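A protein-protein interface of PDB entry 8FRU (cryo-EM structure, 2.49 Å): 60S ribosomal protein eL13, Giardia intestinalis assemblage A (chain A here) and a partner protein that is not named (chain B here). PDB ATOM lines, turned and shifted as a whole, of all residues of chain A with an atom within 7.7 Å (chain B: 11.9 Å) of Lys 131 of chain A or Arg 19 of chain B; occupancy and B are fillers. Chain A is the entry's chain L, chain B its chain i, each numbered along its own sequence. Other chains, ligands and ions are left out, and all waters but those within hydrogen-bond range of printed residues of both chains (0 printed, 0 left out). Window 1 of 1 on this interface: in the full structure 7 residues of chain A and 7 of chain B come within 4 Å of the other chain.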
ATOM      1  N   THR A 105      23.026   9.128   7.366  1.00  0.00           N
ATOM      2  CA  THR A 105      22.736   9.856   6.142  1.00  0.00           C
ATOM      3  C   THR A 105      21.255   9.745   5.789  1.00  0.00           C
ATOM      4  O   THR A 105      20.501   8.960   6.368  1.00  0.00           O
ATOM      5  CB  THR A 105      23.591   9.351   4.977  1.00  0.00           C
ATOM      6  OG1 THR A 105      23.133   8.065   4.557  1.00  0.00           O
ATOM      7  CG2 THR A 105      25.040   9.246   5.374  1.00  0.00           C
ATOM      8  N   LEU A 106      20.841  10.551   4.811  1.00  0.00           N
ATOM      9  CA  LEU A 106      19.436  10.588   4.421  1.00  0.00           C
ATOM     10  C   LEU A 106      19.009   9.323   3.686  1.00  0.00           C
ATOM     11  O   LEU A 106      17.837   8.937   3.755  1.00  0.00           O
ATOM     12  CB  LEU A 106      19.172  11.819   3.559  1.00  0.00           C
ATOM     13  CG  LEU A 106      19.417  13.170   4.231  1.00  0.00           C
ATOM     14  CD1 LEU A 106      19.248  14.299   3.236  1.00  0.00           C
ATOM     15  CD2 LEU A 106      18.493  13.368   5.416  1.00  0.00           C
ATOM     16  N   ARG A 107      19.931   8.666   2.982  1.00  0.00           N
ATOM     17  CA  ARG A 107      19.584   7.421   2.305  1.00  0.00           C
ATOM     18  C   ARG A 107      19.243   6.323   3.299  1.00  0.00           C
ATOM     19  O   ARG A 107      18.308   5.549   3.078  1.00  0.00           O
ATOM     20  CB  ARG A 107      20.721   6.968   1.401  1.00  0.00           C
ATOM     21  CG  ARG A 107      20.673   7.555   0.019  1.00  0.00           C
ATOM     22  CD  ARG A 107      21.388   6.655  -0.951  1.00  0.00           C
ATOM     23  NE  ARG A 107      21.031   5.260  -0.730  1.00  0.00           N
ATOM     24  CZ  ARG A 107      21.365   4.265  -1.538  1.00  0.00           C
ATOM     25  NH1 ARG A 107      22.052   4.477  -2.647  1.00  0.00           N
ATOM     26  NH2 ARG A 107      20.993   3.027  -1.229  1.00  0.00           N
ATOM     27  N   GLU A 108      19.993   6.230   4.394  1.00  0.00           N
ATOM     28  CA  GLU A 108      19.674   5.232   5.406  1.00  0.00           C
ATOM     29  C   GLU A 108      18.302   5.490   6.013  1.00  0.00           C
ATOM     30  O   GLU A 108      17.504   4.558   6.196  1.00  0.00           O
ATOM     31  CB  GLU A 108      20.757   5.227   6.481  1.00  0.00           C
ATOM     32  CG  GLU A 108      22.023   4.495   6.084  1.00  0.00           C
ATOM     33  CD  GLU A 108      23.292   5.255   6.437  1.00  0.00           C
ATOM     34  OE1 GLU A 108      23.281   6.016   7.420  1.00  0.00           O
ATOM     35  OE2 GLU A 108      24.308   5.084   5.737  1.00  0.00           O
ATOM     36  N   ASP A 127      23.291  13.365  10.005  1.00  0.00           N
ATOM     37  CA  ASP A 127      24.401  14.091   9.385  1.00  0.00           C
ATOM     38  C   ASP A 127      24.188  14.165   7.879  1.00  0.00           C
ATOM     39  O   ASP A 127      24.555  13.242   7.144  1.00  0.00           O
ATOM     40  CB  ASP A 127      25.736  13.430   9.715  1.00  0.00           C
ATOM     41  CG  ASP A 127      26.925  14.229   9.225  1.00  0.00           C
ATOM     42  OD1 ASP A 127      26.784  15.448   9.025  1.00  0.00           O
ATOM     43  OD2 ASP A 127      28.004  13.636   9.041  1.00  0.00           O
ATOM     44  N   PRO A 128      23.595  15.252   7.380  1.00  0.00           N
ATOM     45  CA  PRO A 128      23.397  15.393   5.934  1.00  0.00           C
ATOM     46  C   PRO A 128      24.653  15.761   5.157  1.00  0.00           C
ATOM     47  O   PRO A 128      24.595  15.842   3.928  1.00  0.00           O
ATOM     48  CB  PRO A 128      22.348  16.509   5.841  1.00  0.00           C
ATOM     49  CG  PRO A 128      22.538  17.299   7.060  1.00  0.00           C
ATOM     50  CD  PRO A 128      22.995  16.364   8.133  1.00  0.00           C
ATOM     51  N   ARG A 129      25.776  15.999   5.827  1.00  0.00           N
ATOM     52  CA  ARG A 129      27.026  16.273   5.132  1.00  0.00           C
ATOM     53  C   ARG A 129      27.660  15.006   4.569  1.00  0.00           C
ATOM     54  O   ARG A 129      28.298  15.057   3.514  1.00  0.00           O
ATOM     55  CB  ARG A 129      27.988  16.976   6.087  1.00  0.00           C
ATOM     56  CG  ARG A 129      29.232  17.548   5.472  1.00  0.00           C
ATOM     57  CD  ARG A 129      30.116  18.125   6.558  1.00  0.00           C
ATOM     58  NE  ARG A 129      29.482  19.264   7.207  1.00  0.00           N
ATOM     59  CZ  ARG A 129      29.135  19.321   8.486  1.00  0.00           C
ATOM     60  NH1 ARG A 129      29.362  18.314   9.313  1.00  0.00           N
ATOM     61  NH2 ARG A 129      28.547  20.419   8.948  1.00  0.00           N
ATOM     62  N   ARG A 130      27.488  13.873   5.243  1.00  0.00           N
ATOM     63  CA  ARG A 130      28.114  12.627   4.833  1.00  0.00           C
ATOM     64  C   ARG A 130      27.368  11.974   3.677  1.00  0.00           C
ATOM     65  O   ARG A 130      26.136  11.986   3.623  1.00  0.00           O
ATOM     66  CB  ARG A 130      28.184  11.656   6.010  1.00  0.00           C
ATOM     67  CG  ARG A 130      28.814  10.317   5.665  1.00  0.00           C
ATOM     68  CD  ARG A 130      29.150   9.511   6.901  1.00  0.00           C
ATOM     69  NE  ARG A 130      27.954   9.003   7.555  1.00  0.00           N
ATOM     70  CZ  ARG A 130      27.467   7.782   7.393  1.00  0.00           C
ATOM     71  NH1 ARG A 130      28.060   6.901   6.610  1.00  0.00           N
ATOM     72  NH2 ARG A 130      26.355   7.439   8.032  1.00  0.00           N
ATOM     73  N   LYS A 131      28.128  11.393   2.756  1.00  0.00           N
ATOM     74  CA  LYS A 131      27.598  10.653   1.621  1.00  0.00           C
ATOM     75  C   LYS A 131      28.122   9.226   1.665  1.00  0.00           C
ATOM     76  O   LYS A 131      29.292   8.999   1.978  1.00  0.00           O
ATOM     77  CB  LYS A 131      27.995  11.308   0.298  1.00  0.00           C
ATOM     78  CG  LYS A 131      27.536  12.739   0.157  1.00  0.00           C
ATOM     79  CD  LYS A 131      26.077  12.792  -0.237  1.00  0.00           C
ATOM     80  CE  LYS A 131      25.497  14.189  -0.098  1.00  0.00           C
ATOM     81  NZ  LYS A 131      25.944  14.906   1.124  1.00  0.00           N
ATOM     82  N   ASN A 132      27.254   8.267   1.364  1.00  0.00           N
ATOM     83  CA  ASN A 132      27.684   6.879   1.320  1.00  0.00           C
ATOM     84  C   ASN A 132      28.542   6.627   0.089  1.00  0.00           C
ATOM     85  O   ASN A 132      28.316   7.203  -0.976  1.00  0.00           O
ATOM     86  CB  ASN A 132      26.483   5.940   1.320  1.00  0.00           C
ATOM     87  CG  ASN A 132      25.794   5.876   2.661  1.00  0.00           C
ATOM     88  OD1 ASN A 132      24.731   6.457   2.850  1.00  0.00           O
ATOM     89  ND2 ASN A 132      26.398   5.169   3.604  1.00  0.00           N
ATOM     90  N   LYS A 133      29.535   5.758   0.239  1.00  0.00           N
ATOM     91  CA  LYS A 133      30.424   5.412  -0.855  1.00  0.00           C
ATOM     92  C   LYS A 133      30.251   3.987  -1.359  1.00  0.00           C
ATOM     93  O   LYS A 133      30.826   3.643  -2.394  1.00  0.00           O
ATOM     94  CB  LYS A 133      31.879   5.639  -0.434  1.00  0.00           C
ATOM     95  CG  LYS A 133      32.258   7.104  -0.436  1.00  0.00           C
ATOM     96  CD  LYS A 133      32.984   7.514   0.816  1.00  0.00           C
ATOM     97  CE  LYS A 133      33.365   8.977   0.741  1.00  0.00           C
ATOM     98  NZ  LYS A 133      32.356   9.849   1.375  1.00  0.00           N
ATOM     99  N   SER A 134      29.469   3.161  -0.672  1.00  0.00           N
ATOM    100  CA  SER A 134      29.177   1.810  -1.126  1.00  0.00           C
ATOM    101  C   SER A 134      27.873   1.367  -0.486  1.00  0.00           C
ATOM    102  O   SER A 134      27.401   1.971   0.479  1.00  0.00           O
ATOM    103  CB  SER A 134      30.320   0.844  -0.788  1.00  0.00           C
ATOM    104  OG  SER A 134      30.348   0.534   0.589  1.00  0.00           O
ATOM    105  N   SER A 137      27.922  -0.167   3.401  1.00  0.00           N
ATOM    106  CA  SER A 137      27.707   0.776   4.492  1.00  0.00           C
ATOM    107  C   SER A 137      26.228   1.071   4.676  1.00  0.00           C
ATOM    108  O   SER A 137      25.727   1.130   5.809  1.00  0.00           O
ATOM    109  CB  SER A 137      28.476   2.066   4.225  1.00  0.00           C
ATOM    110  OG  SER A 137      28.492   2.358   2.844  1.00  0.00           O
ATOM    111  N   VAL A 138      25.512   1.256   3.569  1.00  0.00           N
ATOM    112  CA  VAL A 138      24.086   1.537   3.644  1.00  0.00           C
ATOM    113  C   VAL A 138      23.361   0.383   4.319  1.00  0.00           C
ATOM    114  O   VAL A 138      22.515   0.588   5.197  1.00  0.00           O
ATOM    115  CB  VAL A 138      23.525   1.819   2.239  1.00  0.00           C
ATOM    116  CG1 VAL A 138      22.029   1.984   2.293  1.00  0.00           C
ATOM    117  CG2 VAL A 138      24.184   3.040   1.641  1.00  0.00           C
ATOM    118  N   VAL B  15      30.941  -2.744  -4.005  1.00  0.00           N
ATOM    119  CA  VAL B  15      30.524  -2.116  -5.252  1.00  0.00           C
ATOM    120  C   VAL B  15      30.335  -0.629  -4.990  1.00  0.00           C
ATOM    121  O   VAL B  15      29.644  -0.240  -4.044  1.00  0.00           O
ATOM    122  CB  VAL B  15      29.248  -2.761  -5.830  1.00  0.00           C
ATOM    123  CG1 VAL B  15      28.017  -2.227  -5.160  1.00  0.00           C
ATOM    124  CG2 VAL B  15      29.169  -2.516  -7.325  1.00  0.00           C
ATOM    125  N   ARG B  16      30.966   0.193  -5.820  1.00  0.00           N
ATOM    126  CA  ARG B  16      31.009   1.627  -5.605  1.00  0.00           C
ATOM    127  C   ARG B  16      29.659   2.272  -5.902  1.00  0.00           C
ATOM    128  O   ARG B  16      28.794   1.703  -6.571  1.00  0.00           O
ATOM    129  CB  ARG B  16      32.095   2.253  -6.482  1.00  0.00           C
ATOM    130  CG  ARG B  16      32.342   3.726  -6.247  1.00  0.00           C
ATOM    131  CD  ARG B  16      33.565   3.966  -5.384  1.00  0.00           C
ATOM    132  NE  ARG B  16      34.125   5.294  -5.603  1.00  0.00           N
ATOM    133  CZ  ARG B  16      33.859   6.357  -4.853  1.00  0.00           C
ATOM    134  NH1 ARG B  16      33.051   6.284  -3.810  1.00  0.00           N
ATOM    135  NH2 ARG B  16      34.415   7.525  -5.163  1.00  0.00           N
ATOM    136  N   ILE B  17      29.488   3.481  -5.380  1.00  0.00           N
ATOM    137  CA  ILE B  17      28.345   4.331  -5.676  1.00  0.00           C
ATOM    138  C   ILE B  17      28.846   5.536  -6.457  1.00  0.00           C
ATOM    139  O   ILE B  17      29.949   6.034  -6.207  1.00  0.00           O
ATOM    140  CB  ILE B  17      27.614   4.771  -4.394  1.00  0.00           C
ATOM    141  CG1 ILE B  17      26.974   3.567  -3.708  1.00  0.00           C
ATOM    142  CG2 ILE B  17      26.579   5.827  -4.716  1.00  0.00           C
ATOM    143  CD1 ILE B  17      26.273   3.902  -2.420  1.00  0.00           C
ATOM    144  N   VAL B  18      28.042   5.998  -7.408  1.00  0.00           N
ATOM    145  CA  VAL B  18      28.425   7.082  -8.305  1.00  0.00           C
ATOM    146  C   VAL B  18      27.500   8.261  -8.056  1.00  0.00           C
ATOM    147  O   VAL B  18      26.272   8.124  -8.132  1.00  0.00           O
ATOM    148  CB  VAL B  18      28.375   6.645  -9.775  1.00  0.00           C
ATOM    149  CG1 VAL B  18      29.593   5.795 -10.110  1.00  0.00           C
ATOM    150  CG2 VAL B  18      27.094   5.878 -10.048  1.00  0.00           C
ATOM    151  N   ARG B  19      28.086   9.415  -7.762  1.00  0.00           N
ATOM    152  CA  ARG B  19      27.339  10.635  -7.521  1.00  0.00           C
ATOM    153  C   ARG B  19      27.270  11.463  -8.800  1.00  0.00           C
ATOM    154  O   ARG B  19      27.859  11.123  -9.827  1.00  0.00           O
ATOM    155  CB  ARG B  19      27.974  11.427  -6.378  1.00  0.00           C
ATOM    156  CG  ARG B  19      29.490  11.478  -6.437  1.00  0.00           C
ATOM    157  CD  ARG B  19      30.076  11.986  -5.132  1.00  0.00           C
ATOM    158  NE  ARG B  19      29.346  13.131  -4.600  1.00  0.00           N
ATOM    159  CZ  ARG B  19      29.548  13.653  -3.397  1.00  0.00           C
ATOM    160  NH1 ARG B  19      30.455  13.158  -2.572  1.00  0.00           N
ATOM    161  NH2 ARG B  19      28.829  14.704  -3.017  1.00  0.00           N
ATOM    162  N   LYS B  20      26.531  12.566  -8.731  1.00  0.00           N
ATOM    163  CA  LYS B  20      26.400  13.493  -9.853  1.00  0.00           C
ATOM    164  C   LYS B  20      25.961  12.782 -11.130  1.00  0.00           C
ATOM    165  O   LYS B  20      24.849  12.262 -11.209  1.00  0.00           O
ATOM    166  CB  LYS B  20      27.721  14.230 -10.093  1.00  0.00           C
ATOM    167  CG  LYS B  20      27.686  15.167 -11.283  1.00  0.00           C
ATOM    168  CD  LYS B  20      28.525  14.637 -12.435  1.00  0.00           C
ATOM    169  CE  LYS B  20      28.775  15.716 -13.474  1.00  0.00           C
ATOM    170  NZ  LYS B  20      29.599  16.838 -12.938  1.00  0.00           N
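Of the 6 printed residues of chain B, 4 touch a printed residue of chain A. Hydrophobic or aromatic side chains of chain B that line the printed part of chain A: Ile 17. Of the 14 printed residues of chain A, 3 touch a printed residue of chain B. Printed residues of chain A that touch a printed residue of chain B: Lys 131, Lys 133 and Ser 134. Among the printed residues, 5 pairs touch across the chains. Among the printed residues, no Asp or Glu carboxylate lies within 4 Å of a Lys or Arg side-chain nitrogen of the other chain.
Among the printed residues, merely in contact across the chains: Lys 131 of chain A with Arg 19 of chain B, Lys 133 of chain A with Arg 16 of chain B, Ser 134 of chain A with Val 15 of chain B and Ser 134 of chain A with Ile 17 of chain B.
The side-chain hydroxyl (OG) of Ser 137 of chain A is in hydrogen-bond range of the backbone carbonyl oxygen (O) of Ser 134 of chain A (2.6 Å). The side-chain amino group (NZ) of Lys 133 of chain A lies within hydrogen-bond range of the backbone carbonyl oxygen (O) of Lys 131 of chain A, 3.2 Å away. The side-chain amino group (NZ) of Lys 131 of chain A is in hydrogen-bond range of the backbone carbonyl oxygen (O) of Arg 129 of chain A (3.4 Å). NZ of Lys 131 of chain A sits at hydrogen-bond distance from O of Pro 128 of chain A.
O of Lys 133 of chain A is in hydrogen-bond range of N of Ile 17 of chain B (3.3 Å).
No residue of chain B comes within 4 Å of Pro 128 of chain A. Printed residues of chain B within 4 Å of Lys 131 of chain A: Arg 19 (3.95 Å). Asn 132 of chain A touches none of the printed residues of chain B. Printed residues of chain B within 4 Å of Ser 134 of chain A: Val 15 (3.5 Å) and Ile 17 (3.6 Å). Printed residues of chain A within 4 Å of Val 15 of chain B: Ser 134 (3.5 Å). Of the printed residues of chain A, Arg 16 of chain B touches Lys 133 (3.6 Å). The nearest residue of chain A that does not touch Arg 19 of chain B is Lys 133 of chain A (5.5 Å). The nearest printed residue of chain A that does not touch Ile 17 of chain B is Asn 132 of chain A (4.1 Å).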
